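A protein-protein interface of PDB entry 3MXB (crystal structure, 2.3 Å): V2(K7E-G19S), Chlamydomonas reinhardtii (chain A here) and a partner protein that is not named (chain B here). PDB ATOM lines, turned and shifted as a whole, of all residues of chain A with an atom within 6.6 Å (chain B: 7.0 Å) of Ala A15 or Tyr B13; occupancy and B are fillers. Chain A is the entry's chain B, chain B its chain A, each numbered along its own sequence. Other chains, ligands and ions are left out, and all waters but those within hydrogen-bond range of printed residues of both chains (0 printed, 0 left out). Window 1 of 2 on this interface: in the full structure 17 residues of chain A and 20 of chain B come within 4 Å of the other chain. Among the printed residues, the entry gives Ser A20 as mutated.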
ATOM      1  N   PHE A  10     -27.387 -13.668 -19.331  1.00  0.00           N
ATOM      2  CA  PHE A  10     -26.431 -12.924 -20.124  1.00  0.00           C
ATOM      3  C   PHE A  10     -27.085 -11.625 -20.583  1.00  0.00           C
ATOM      4  O   PHE A  10     -26.540 -10.535 -20.384  1.00  0.00           O
ATOM      5  CB  PHE A  10     -25.973 -13.770 -21.325  1.00  0.00           C
ATOM      6  CG  PHE A  10     -25.193 -13.001 -22.346  1.00  0.00           C
ATOM      7  CD1 PHE A  10     -23.896 -12.579 -22.077  1.00  0.00           C
ATOM      8  CD2 PHE A  10     -25.753 -12.701 -23.580  1.00  0.00           C
ATOM      9  CE1 PHE A  10     -23.174 -11.854 -23.016  1.00  0.00           C
ATOM     10  CE2 PHE A  10     -25.036 -11.978 -24.535  1.00  0.00           C
ATOM     11  CZ  PHE A  10     -23.741 -11.556 -24.250  1.00  0.00           C
ATOM     12  N   LEU A  11     -28.276 -11.756 -21.160  1.00  0.00           N
ATOM     13  CA  LEU A  11     -29.006 -10.624 -21.704  1.00  0.00           C
ATOM     14  C   LEU A  11     -29.466  -9.612 -20.645  1.00  0.00           C
ATOM     15  O   LEU A  11     -29.490  -8.419 -20.920  1.00  0.00           O
ATOM     16  CB  LEU A  11     -30.196 -11.100 -22.539  1.00  0.00           C
ATOM     17  CG  LEU A  11     -29.928 -11.727 -23.910  1.00  0.00           C
ATOM     18  CD1 LEU A  11     -31.181 -12.488 -24.401  1.00  0.00           C
ATOM     19  CD2 LEU A  11     -29.486 -10.702 -24.937  1.00  0.00           C
ATOM     20  N   LEU A  12     -29.844 -10.091 -19.460  1.00  0.00           N
ATOM     21  CA  LEU A  12     -30.220  -9.205 -18.351  1.00  0.00           C
ATOM     22  C   LEU A  12     -29.058  -8.323 -17.886  1.00  0.00           C
ATOM     23  O   LEU A  12     -29.207  -7.104 -17.750  1.00  0.00           O
ATOM     24  CB  LEU A  12     -30.742 -10.009 -17.156  1.00  0.00           C
ATOM     25  CG  LEU A  12     -32.205 -10.470 -17.211  1.00  0.00           C
ATOM     26  CD1 LEU A  12     -32.483 -11.574 -16.179  1.00  0.00           C
ATOM     27  CD2 LEU A  12     -33.141  -9.281 -17.011  1.00  0.00           C
ATOM     28  N   TYR A  13     -27.913  -8.945 -17.616  1.00  0.00           N
ATOM     29  CA  TYR A  13     -26.733  -8.202 -17.192  1.00  0.00           C
ATOM     30  C   TYR A  13     -26.268  -7.244 -18.296  1.00  0.00           C
ATOM     31  O   TYR A  13     -25.966  -6.081 -18.041  1.00  0.00           O
ATOM     32  CB  TYR A  13     -25.596  -9.152 -16.819  1.00  0.00           C
ATOM     33  CG  TYR A  13     -24.322  -8.416 -16.488  1.00  0.00           C
ATOM     34  CD1 TYR A  13     -23.982  -8.149 -15.173  1.00  0.00           C
ATOM     35  CD2 TYR A  13     -23.472  -7.967 -17.494  1.00  0.00           C
ATOM     36  CE1 TYR A  13     -22.831  -7.474 -14.859  1.00  0.00           C
ATOM     37  CE2 TYR A  13     -22.313  -7.278 -17.192  1.00  0.00           C
ATOM     38  CZ  TYR A  13     -22.002  -7.029 -15.871  1.00  0.00           C
ATOM     39  OH  TYR A  13     -20.854  -6.355 -15.548  1.00  0.00           O
ATOM     40  N   LEU A  14     -26.217  -7.747 -19.526  1.00  0.00           N
ATOM     41  CA  LEU A  14     -25.801  -6.940 -20.660  1.00  0.00           C
ATOM     42  C   LEU A  14     -26.714  -5.726 -20.886  1.00  0.00           C
ATOM     43  O   LEU A  14     -26.224  -4.639 -21.174  1.00  0.00           O
ATOM     44  CB  LEU A  14     -25.705  -7.783 -21.924  1.00  0.00           C
ATOM     45  CG  LEU A  14     -25.211  -7.062 -23.180  1.00  0.00           C
ATOM     46  CD1 LEU A  14     -23.938  -6.264 -22.867  1.00  0.00           C
ATOM     47  CD2 LEU A  14     -24.987  -8.053 -24.332  1.00  0.00           C
ATOM     48  N   ALA A  15     -28.030  -5.896 -20.745  1.00  0.00           N
ATOM     49  CA  ALA A  15     -28.914  -4.740 -20.879  1.00  0.00           C
ATOM     50  C   ALA A  15     -28.592  -3.629 -19.855  1.00  0.00           C
ATOM     51  O   ALA A  15     -28.608  -2.453 -20.199  1.00  0.00           O
ATOM     52  CB  ALA A  15     -30.365  -5.142 -20.791  1.00  0.00           C
ATOM     53  N   GLY A  16     -28.343  -4.008 -18.601  1.00  0.00           N
ATOM     54  CA  GLY A  16     -27.957  -3.058 -17.576  1.00  0.00           C
ATOM     55  C   GLY A  16     -26.655  -2.357 -17.936  1.00  0.00           C
ATOM     56  O   GLY A  16     -26.524  -1.138 -17.776  1.00  0.00           O
ATOM     57  N   PHE A  17     -25.698  -3.124 -18.448  1.00  0.00           N
ATOM     58  CA  PHE A  17     -24.419  -2.575 -18.828  1.00  0.00           C
ATOM     59  C   PHE A  17     -24.534  -1.657 -20.045  1.00  0.00           C
ATOM     60  O   PHE A  17     -23.828  -0.652 -20.134  1.00  0.00           O
ATOM     61  CB  PHE A  17     -23.368  -3.664 -19.074  1.00  0.00           C
ATOM     62  CG  PHE A  17     -21.966  -3.150 -18.985  1.00  0.00           C
ATOM     63  CD1 PHE A  17     -21.334  -3.031 -17.755  1.00  0.00           C
ATOM     64  CD2 PHE A  17     -21.292  -2.729 -20.115  1.00  0.00           C
ATOM     65  CE1 PHE A  17     -20.038  -2.527 -17.667  1.00  0.00           C
ATOM     66  CE2 PHE A  17     -20.001  -2.227 -20.030  1.00  0.00           C
ATOM     67  CZ  PHE A  17     -19.378  -2.120 -18.805  1.00  0.00           C
ATOM     68  N   VAL A  18     -25.435  -2.005 -20.960  1.00  0.00           N
ATOM     69  CA  VAL A  18     -25.687  -1.222 -22.165  1.00  0.00           C
ATOM     70  C   VAL A  18     -26.406   0.100 -21.856  1.00  0.00           C
ATOM     71  O   VAL A  18     -25.991   1.185 -22.321  1.00  0.00           O
ATOM     72  CB  VAL A  18     -26.472  -2.032 -23.213  1.00  0.00           C
ATOM     73  CG1 VAL A  18     -27.117  -1.104 -24.283  1.00  0.00           C
ATOM     74  CG2 VAL A  18     -25.570  -3.072 -23.846  1.00  0.00           C
ATOM     75  N   ASP A  19     -27.471   0.001 -21.068  1.00  0.00           N
ATOM     76  CA  ASP A  19     -28.178   1.170 -20.546  1.00  0.00           C
ATOM     77  C   ASP A  19     -27.245   2.150 -19.801  1.00  0.00           C
ATOM     78  O   ASP A  19     -27.527   3.345 -19.750  1.00  0.00           O
ATOM     79  CB  ASP A  19     -29.316   0.726 -19.591  1.00  0.00           C
ATOM     80  CG  ASP A  19     -30.614   0.390 -20.327  1.00  0.00           C
ATOM     81  OD1 ASP A  19     -30.721   0.684 -21.536  1.00  0.00           O
ATOM     82  OD2 ASP A  19     -31.534  -0.161 -19.684  1.00  0.00           O
ATOM     83  N   SER A  20     -26.166   1.642 -19.195  1.00  0.00           N
ATOM     84  CA  SER A  20     -25.216   2.498 -18.476  1.00  0.00           C
ATOM     85  C   SER A  20     -24.073   2.992 -19.373  1.00  0.00           C
ATOM     86  O   SER A  20     -23.926   4.181 -19.587  1.00  0.00           O
ATOM     87  CB  SER A  20     -24.666   1.828 -17.201  1.00  0.00           C
ATOM     88  OG  SER A  20     -24.029   0.578 -17.449  1.00  0.00           O
ATOM     89  N   LEU A  92     -32.184  -8.517 -27.179  1.00  0.00           N
ATOM     90  CA  LEU A  92     -31.780  -7.658 -26.083  1.00  0.00           C
ATOM     91  C   LEU A  92     -32.894  -6.716 -25.623  1.00  0.00           C
ATOM     92  O   LEU A  92     -33.007  -6.418 -24.436  1.00  0.00           O
ATOM     93  CB  LEU A  92     -30.532  -6.859 -26.457  1.00  0.00           C
ATOM     94  CG  LEU A  92     -29.952  -6.029 -25.314  1.00  0.00           C
ATOM     95  CD1 LEU A  92     -29.304  -6.943 -24.301  1.00  0.00           C
ATOM     96  CD2 LEU A  92     -28.946  -5.009 -25.843  1.00  0.00           C
ATOM     97  N   PRO A  94     -36.126  -6.556 -24.911  1.00  0.00           N
ATOM     98  CA  PRO A  94     -37.093  -6.703 -23.818  1.00  0.00           C
ATOM     99  C   PRO A  94     -36.524  -6.280 -22.461  1.00  0.00           C
ATOM    100  O   PRO A  94     -37.264  -5.875 -21.563  1.00  0.00           O
ATOM    101  CB  PRO A  94     -37.402  -8.214 -23.813  1.00  0.00           C
ATOM    102  CG  PRO A  94     -37.097  -8.666 -25.206  1.00  0.00           C
ATOM    103  CD  PRO A  94     -35.934  -7.808 -25.660  1.00  0.00           C
ATOM    104  N   PHE A  95     -35.214  -6.370 -22.306  1.00  0.00           N
ATOM    105  CA  PHE A  95     -34.618  -6.105 -21.007  1.00  0.00           C
ATOM    106  C   PHE A  95     -34.055  -4.687 -20.864  1.00  0.00           C
ATOM    107  O   PHE A  95     -33.630  -4.287 -19.786  1.00  0.00           O
ATOM    108  CB  PHE A  95     -33.569  -7.174 -20.694  1.00  0.00           C
ATOM    109  CG  PHE A  95     -34.062  -8.568 -20.935  1.00  0.00           C
ATOM    110  CD1 PHE A  95     -34.947  -9.163 -20.043  1.00  0.00           C
ATOM    111  CD2 PHE A  95     -33.675  -9.271 -22.070  1.00  0.00           C
ATOM    112  CE1 PHE A  95     -35.421 -10.437 -20.263  1.00  0.00           C
ATOM    113  CE2 PHE A  95     -34.152 -10.550 -22.306  1.00  0.00           C
ATOM    114  CZ  PHE A  95     -35.019 -11.137 -21.396  1.00  0.00           C
ATOM    115  N   LEU A  96     -34.069  -3.919 -21.946  1.00  0.00           N
ATOM    116  CA  LEU A  96     -33.562  -2.556 -21.881  1.00  0.00           C
ATOM    117  C   LEU A  96     -34.552  -1.640 -21.172  1.00  0.00           C
ATOM    118  O   LEU A  96     -35.768  -1.754 -21.346  1.00  0.00           O
ATOM    119  CB  LEU A  96     -33.247  -2.024 -23.281  1.00  0.00           C
ATOM    120  CG  LEU A  96     -32.099  -2.738 -24.001  1.00  0.00           C
ATOM    121  CD1 LEU A  96     -32.093  -2.377 -25.493  1.00  0.00           C
ATOM    122  CD2 LEU A  96     -30.758  -2.415 -23.337  1.00  0.00           C
ATOM    123  N   LYS A  97     -34.026  -0.725 -20.373  1.00  0.00           N
ATOM    124  CA  LYS A  97     -34.862   0.231 -19.680  1.00  0.00           C
ATOM    125  C   LYS A  97     -34.654   1.648 -20.202  1.00  0.00           C
ATOM    126  O   LYS A  97     -35.621   2.320 -20.548  1.00  0.00           O
ATOM    127  CB  LYS A  97     -34.667   0.119 -18.170  1.00  0.00           C
ATOM    128  CG  LYS A  97     -35.185  -1.217 -17.626  1.00  0.00           C
ATOM    129  CD  LYS A  97     -35.093  -1.316 -16.115  1.00  0.00           C
ATOM    130  CE  LYS A  97     -35.814  -2.569 -15.600  1.00  0.00           C
ATOM    131  NZ  LYS A  97     -35.820  -2.654 -14.110  1.00  0.00           N
ATOM    132  N   LEU A  98     -33.407   2.097 -20.309  1.00  0.00           N
ATOM    133  CA  LEU A  98     -33.166   3.456 -20.789  1.00  0.00           C
ATOM    134  C   LEU A  98     -33.112   3.549 -22.321  1.00  0.00           C
ATOM    135  O   LEU A  98     -33.397   4.598 -22.892  1.00  0.00           O
ATOM    136  CB  LEU A  98     -31.896   4.063 -20.154  1.00  0.00           C
ATOM    137  CG  LEU A  98     -31.871   4.243 -18.630  1.00  0.00           C
ATOM    138  CD1 LEU A  98     -30.530   4.820 -18.151  1.00  0.00           C
ATOM    139  CD2 LEU A  98     -33.021   5.112 -18.150  1.00  0.00           C
ATOM    140  N   LYS A  99     -32.738   2.462 -22.988  1.00  0.00           N
ATOM    141  CA  LYS A  99     -32.556   2.502 -24.434  1.00  0.00           C
ATOM    142  C   LYS A  99     -33.523   1.587 -25.187  1.00  0.00           C
ATOM    143  O   LYS A  99     -33.278   1.233 -26.338  1.00  0.00           O
ATOM    144  CB  LYS A  99     -31.102   2.143 -24.788  1.00  0.00           C
ATOM    145  CG  LYS A  99     -30.063   3.105 -24.197  1.00  0.00           C
ATOM    146  CD  LYS A  99     -28.634   2.649 -24.483  1.00  0.00           C
ATOM    147  CE  LYS A  99     -27.606   3.550 -23.788  1.00  0.00           C
ATOM    148  NZ  LYS A  99     -27.665   4.939 -24.313  1.00  0.00           N
ATOM    149  N   LYS B   8     -34.592 -11.845  -8.888  1.00  0.00           N
ATOM    150  CA  LYS B   8     -33.335 -12.194  -9.539  1.00  0.00           C
ATOM    151  C   LYS B   8     -33.122 -11.471 -10.877  1.00  0.00           C
ATOM    152  O   LYS B   8     -32.005 -11.091 -11.197  1.00  0.00           O
ATOM    153  CB  LYS B   8     -33.222 -13.716  -9.720  1.00  0.00           C
ATOM    154  CG  LYS B   8     -31.910 -14.184 -10.338  1.00  0.00           C
ATOM    155  CD  LYS B   8     -31.848 -15.709 -10.397  1.00  0.00           C
ATOM    156  CE  LYS B   8     -30.540 -16.189 -10.996  1.00  0.00           C
ATOM    157  NZ  LYS B   8     -30.514 -17.667 -11.149  1.00  0.00           N
ATOM    158  N   LYS B   9     -34.187 -11.311 -11.660  1.00  0.00           N
ATOM    159  CA  LYS B   9     -34.119 -10.573 -12.917  1.00  0.00           C
ATOM    160  C   LYS B   9     -33.633  -9.162 -12.648  1.00  0.00           C
ATOM    161  O   LYS B   9     -32.880  -8.599 -13.433  1.00  0.00           O
ATOM    162  CB  LYS B   9     -35.495 -10.503 -13.596  1.00  0.00           C
ATOM    163  CG  LYS B   9     -35.851 -11.708 -14.449  1.00  0.00           C
ATOM    164  CD  LYS B   9     -37.349 -11.765 -14.710  1.00  0.00           C
ATOM    165  CE  LYS B   9     -37.779 -10.792 -15.796  1.00  0.00           C
ATOM    166  NZ  LYS B   9     -37.835 -11.461 -17.125  1.00  0.00           N
ATOM    167  N   PHE B  10     -34.078  -8.612 -11.523  1.00  0.00           N
ATOM    168  CA  PHE B  10     -33.797  -7.235 -11.133  1.00  0.00           C
ATOM    169  C   PHE B  10     -32.334  -7.091 -10.718  1.00  0.00           C
ATOM    170  O   PHE B  10     -31.659  -6.139 -11.120  1.00  0.00           O
ATOM    171  CB  PHE B  10     -34.761  -6.813 -10.016  1.00  0.00           C
ATOM    172  CG  PHE B  10     -34.282  -5.663  -9.176  1.00  0.00           C
ATOM    173  CD1 PHE B  10     -34.515  -4.351  -9.568  1.00  0.00           C
ATOM    174  CD2 PHE B  10     -33.624  -5.893  -7.979  1.00  0.00           C
ATOM    175  CE1 PHE B  10     -34.081  -3.294  -8.788  1.00  0.00           C
ATOM    176  CE2 PHE B  10     -33.181  -4.840  -7.197  1.00  0.00           C
ATOM    177  CZ  PHE B  10     -33.413  -3.537  -7.600  1.00  0.00           C
ATOM    178  N   LEU B  11     -31.837  -8.064  -9.957  1.00  0.00           N
ATOM    179  CA  LEU B  11     -30.456  -8.038  -9.505  1.00  0.00           C
ATOM    180  C   LEU B  11     -29.470  -8.136 -10.667  1.00  0.00           C
ATOM    181  O   LEU B  11     -28.413  -7.514 -10.638  1.00  0.00           O
ATOM    182  CB  LEU B  11     -30.188  -9.149  -8.493  1.00  0.00           C
ATOM    183  CG  LEU B  11     -30.881  -9.000  -7.138  1.00  0.00           C
ATOM    184  CD1 LEU B  11     -30.790 -10.315  -6.356  1.00  0.00           C
ATOM    185  CD2 LEU B  11     -30.306  -7.818  -6.334  1.00  0.00           C
ATOM    186  N   LEU B  12     -29.820  -8.915 -11.685  1.00  0.00           N
ATOM    187  CA  LEU B  12     -28.957  -9.082 -12.852  1.00  0.00           C
ATOM    188  C   LEU B  12     -28.875  -7.782 -13.639  1.00  0.00           C
ATOM    189  O   LEU B  12     -27.785  -7.321 -13.965  1.00  0.00           O
ATOM    190  CB  LEU B  12     -29.469 -10.184 -13.782  1.00  0.00           C
ATOM    191  CG  LEU B  12     -29.019 -11.640 -13.619  1.00  0.00           C
ATOM    192  CD1 LEU B  12     -27.509 -11.766 -13.705  1.00  0.00           C
ATOM    193  CD2 LEU B  12     -29.529 -12.217 -12.328  1.00  0.00           C
ATOM    194  N   TYR B  13     -30.038  -7.213 -13.956  1.00  0.00           N
ATOM    195  CA  TYR B  13     -30.084  -5.964 -14.683  1.00  0.00           C
ATOM    196  C   TYR B  13     -29.282  -4.936 -13.910  1.00  0.00           C
ATOM    197  O   TYR B  13     -28.387  -4.292 -14.455  1.00  0.00           O
ATOM    198  CB  TYR B  13     -31.508  -5.445 -14.861  1.00  0.00           C
ATOM    199  CG  TYR B  13     -31.507  -4.071 -15.507  1.00  0.00           C
ATOM    200  CD1 TYR B  13     -31.540  -3.930 -16.899  1.00  0.00           C
ATOM    201  CD2 TYR B  13     -31.416  -2.917 -14.734  1.00  0.00           C
ATOM    202  CE1 TYR B  13     -31.534  -2.672 -17.498  1.00  0.00           C
ATOM    203  CE2 TYR B  13     -31.384  -1.657 -15.323  1.00  0.00           C
ATOM    204  CZ  TYR B  13     -31.438  -1.542 -16.705  1.00  0.00           C
ATOM    205  OH  TYR B  13     -31.418  -0.299 -17.286  1.00  0.00           O
ATOM    206  N   LEU B  14     -29.609  -4.811 -12.628  1.00  0.00           N
ATOM    207  CA  LEU B  14     -28.981  -3.826 -11.775  1.00  0.00           C
ATOM    208  C   LEU B  14     -27.463  -3.990 -11.702  1.00  0.00           C
ATOM    209  O   LEU B  14     -26.730  -3.000 -11.720  1.00  0.00           O
ATOM    210  CB  LEU B  14     -29.596  -3.866 -10.383  1.00  0.00           C
ATOM    211  CG  LEU B  14     -29.047  -2.829  -9.407  1.00  0.00           C
ATOM    212  CD1 LEU B  14     -29.124  -1.419 -10.018  1.00  0.00           C
ATOM    213  CD2 LEU B  14     -29.793  -2.896  -8.074  1.00  0.00           C
ATOM    214  N   ALA B  15     -26.998  -5.236 -11.628  1.00  0.00           N
ATOM    215  CA  ALA B  15     -25.566  -5.520 -11.598  1.00  0.00           C
ATOM    216  C   ALA B  15     -24.860  -4.992 -12.855  1.00  0.00           C
ATOM    217  O   ALA B  15     -23.725  -4.533 -12.788  1.00  0.00           O
ATOM    218  CB  ALA B  15     -25.309  -7.021 -11.433  1.00  0.00           C
ATOM    219  N   GLY B  16     -25.525  -5.087 -13.999  1.00  0.00           N
ATOM    220  CA  GLY B  16     -24.973  -4.553 -15.232  1.00  0.00           C
ATOM    221  C   GLY B  16     -24.912  -3.030 -15.171  1.00  0.00           C
ATOM    222  O   GLY B  16     -23.944  -2.399 -15.646  1.00  0.00           O
ATOM    223  N   PHE B  17     -25.939  -2.441 -14.563  1.00  0.00           N
ATOM    224  CA  PHE B  17     -26.024  -0.987 -14.494  1.00  0.00           C
ATOM    225  C   PHE B  17     -25.006  -0.460 -13.500  1.00  0.00           C
ATOM    226  O   PHE B  17     -24.346   0.549 -13.748  1.00  0.00           O
ATOM    227  CB  PHE B  17     -27.437  -0.509 -14.141  1.00  0.00           C
ATOM    228  CG  PHE B  17     -27.736   0.888 -14.630  1.00  0.00           C
ATOM    229  CD1 PHE B  17     -28.266   1.098 -15.899  1.00  0.00           C
ATOM    230  CD2 PHE B  17     -27.447   1.993 -13.844  1.00  0.00           C
ATOM    231  CE1 PHE B  17     -28.528   2.380 -16.353  1.00  0.00           C
ATOM    232  CE2 PHE B  17     -27.690   3.280 -14.306  1.00  0.00           C
ATOM    233  CZ  PHE B  17     -28.240   3.468 -15.557  1.00  0.00           C
ATOM    234  N   VAL B  18     -24.864  -1.163 -12.382  1.00  0.00           N
ATOM    235  CA  VAL B  18     -23.875  -0.791 -11.376  1.00  0.00           C
ATOM    236  C   VAL B  18     -22.441  -0.900 -11.926  1.00  0.00           C
ATOM    237  O   VAL B  18     -21.608  -0.024 -11.677  1.00  0.00           O
ATOM    238  CB  VAL B  18     -24.030  -1.628 -10.078  1.00  0.00           C
ATOM    239  CG1 VAL B  18     -22.806  -1.495  -9.204  1.00  0.00           C
ATOM    240  CG2 VAL B  18     -25.280  -1.205  -9.320  1.00  0.00           C
ATOM    241  N   ASP B  19     -22.157  -1.962 -12.676  1.00  0.00           N
ATOM    242  CA  ASP B  19     -20.839  -2.105 -13.289  1.00  0.00           C
ATOM    243  C   ASP B  19     -20.600  -0.999 -14.319  1.00  0.00           C
ATOM    244  O   ASP B  19     -19.464  -0.650 -14.598  1.00  0.00           O
ATOM    245  CB  ASP B  19     -20.659  -3.493 -13.924  1.00  0.00           C
ATOM    246  CG  ASP B  19     -20.231  -4.562 -12.902  1.00  0.00           C
ATOM    247  OD1 ASP B  19     -19.724  -4.198 -11.817  1.00  0.00           O
ATOM    248  OD2 ASP B  19     -20.394  -5.765 -13.184  1.00  0.00           O
ATOM    249  N   PHE B  55     -35.279   7.545 -12.900  1.00  0.00           N
ATOM    250  CA  PHE B  55     -34.647   6.238 -12.881  1.00  0.00           C
ATOM    251  C   PHE B  55     -33.976   5.954 -11.523  1.00  0.00           C
ATOM    252  O   PHE B  55     -34.068   4.860 -11.005  1.00  0.00           O
ATOM    253  CB  PHE B  55     -33.649   6.129 -14.025  1.00  0.00           C
ATOM    254  CG  PHE B  55     -33.161   4.729 -14.280  1.00  0.00           C
ATOM    255  CD1 PHE B  55     -33.847   3.891 -15.135  1.00  0.00           C
ATOM    256  CD2 PHE B  55     -32.007   4.266 -13.685  1.00  0.00           C
ATOM    257  CE1 PHE B  55     -33.390   2.613 -15.390  1.00  0.00           C
ATOM    258  CE2 PHE B  55     -31.551   2.994 -13.936  1.00  0.00           C
ATOM    259  CZ  PHE B  55     -32.247   2.166 -14.789  1.00  0.00           C
ATOM    260  N   LEU B  92     -26.453  -8.598  -4.367  1.00  0.00           N
ATOM    261  CA  LEU B  92     -26.022  -8.102  -5.669  1.00  0.00           C
ATOM    262  C   LEU B  92     -24.737  -8.790  -6.124  1.00  0.00           C
ATOM    263  O   LEU B  92     -24.565  -9.116  -7.304  1.00  0.00           O
ATOM    264  CB  LEU B  92     -25.796  -6.588  -5.617  1.00  0.00           C
ATOM    265  CG  LEU B  92     -25.464  -5.984  -6.976  1.00  0.00           C
ATOM    266  CD1 LEU B  92     -26.553  -6.352  -7.941  1.00  0.00           C
ATOM    267  CD2 LEU B  92     -25.288  -4.471  -6.897  1.00  0.00           C
ATOM    268  N   PHE B  95     -23.716 -11.330  -8.978  1.00  0.00           N
ATOM    269  CA  PHE B  95     -23.963 -10.981 -10.375  1.00  0.00           C
ATOM    270  C   PHE B  95     -23.006  -9.933 -10.932  1.00  0.00           C
ATOM    271  O   PHE B  95     -22.926  -9.746 -12.146  1.00  0.00           O
ATOM    272  CB  PHE B  95     -25.416 -10.548 -10.570  1.00  0.00           C
ATOM    273  CG  PHE B  95     -26.395 -11.525 -10.015  1.00  0.00           C
ATOM    274  CD1 PHE B  95     -26.546 -12.782 -10.601  1.00  0.00           C
ATOM    275  CD2 PHE B  95     -27.137 -11.214  -8.889  1.00  0.00           C
ATOM    276  CE1 PHE B  95     -27.434 -13.705 -10.080  1.00  0.00           C
ATOM    277  CE2 PHE B  95     -28.031 -12.135  -8.360  1.00  0.00           C
ATOM    278  CZ  PHE B  95     -28.181 -13.380  -8.958  1.00  0.00           C
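OD2 of Asp A19 sits at hydrogen-bond distance from OH of Tyr B13 (2.4 Å). O of Gly B16 lies close to N of Phe A17 (3.4 Å). The side-chain hydroxyl (OG) of Ser A20 sits at hydrogen-bond distance from the backbone carbonyl oxygen (O) of Gly B16, at 3.5 Å. OH of Tyr A13 sits at hydrogen-bond distance from OD2 of Asp B19, 2.5 Å away.
OG of Ser A20 lies within hydrogen-bond range of O of Gly A16, 3.0 Å away. The backbone carbonyl oxygen of Phe A17 lies within hydrogen-bond range of the side-chain hydroxyl of Ser A20, 3.0 Å away. N of Lys A97 is in hydrogen-bond range of OD2 of Asp A19, 2.6 Å away. The backbone NH (N) of Leu A98 is in hydrogen-bond range of the side-chain carboxylate (OD2) of Asp A19, at 3.0 Å. N of Lys A99 lies within hydrogen-bond range of OD1 of Asp A19.
CD2 of Leu A12 touches O of Lys B9, at 3.7 Å. Leu B12 touches Leu A12. CA of Tyr B13 touches O of Leu A12, at 3.4 Å. O of Leu B12 touches CA of Tyr A13 (3.5 Å). Ala A15 touches Tyr B13 (C to CE1, 3.9 Å). CA of Gly A16 touches O of Tyr B13, at 3.4 Å. C of Gly A16 touches C of Gly B16, 3.3 Å away. O of Phe B17 touches CB of Ser A20 (3.7 Å). Phe A95 touches Tyr B13. Leu A98 touches Phe B55 (CD2 to CD1, 3.4 Å).
Ala A15 touches just one residue of chain B: Tyr B13. Tyr B13 touches just these residues of chain A: Leu A12, Ala A15, Gly A16, Asp A19, Phe A95 and Lys A97. Printed residues of chain A within 4 Å of Phe B17: Gly A16 (3.3 Å), Phe A17 (3.95 Å), Asp A19 (3.7 Å), Ser A20 (3.7 Å) and Leu A98 (3.6 Å). Printed residues of chain B within 4 Å of Leu A12: Lys B9 (3.7 Å), Leu B12 (3.6 Å) and Tyr B13 (3.4 Å). Of the printed residues of chain B, Leu A98 touches Phe B17 (3.6 Å) and Phe B55 (3.4 Å). Of the printed residues of chain B, Tyr A13 touches Leu B12, Ala B15, Gly B16, Asp B19 and Phe B95. The nearest residue of chain A that does not touch Tyr B13 is Leu A98 (4.3 Å).
Of the 18 printed residues of chain A, 10 touch a printed residue of chain B. Among the printed residues, 24 pairs touch across the chains. Among the printed residues, no Asp or Glu carboxylate lies within 4 Å of a Lys or Arg side-chain nitrogen of the other chain.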
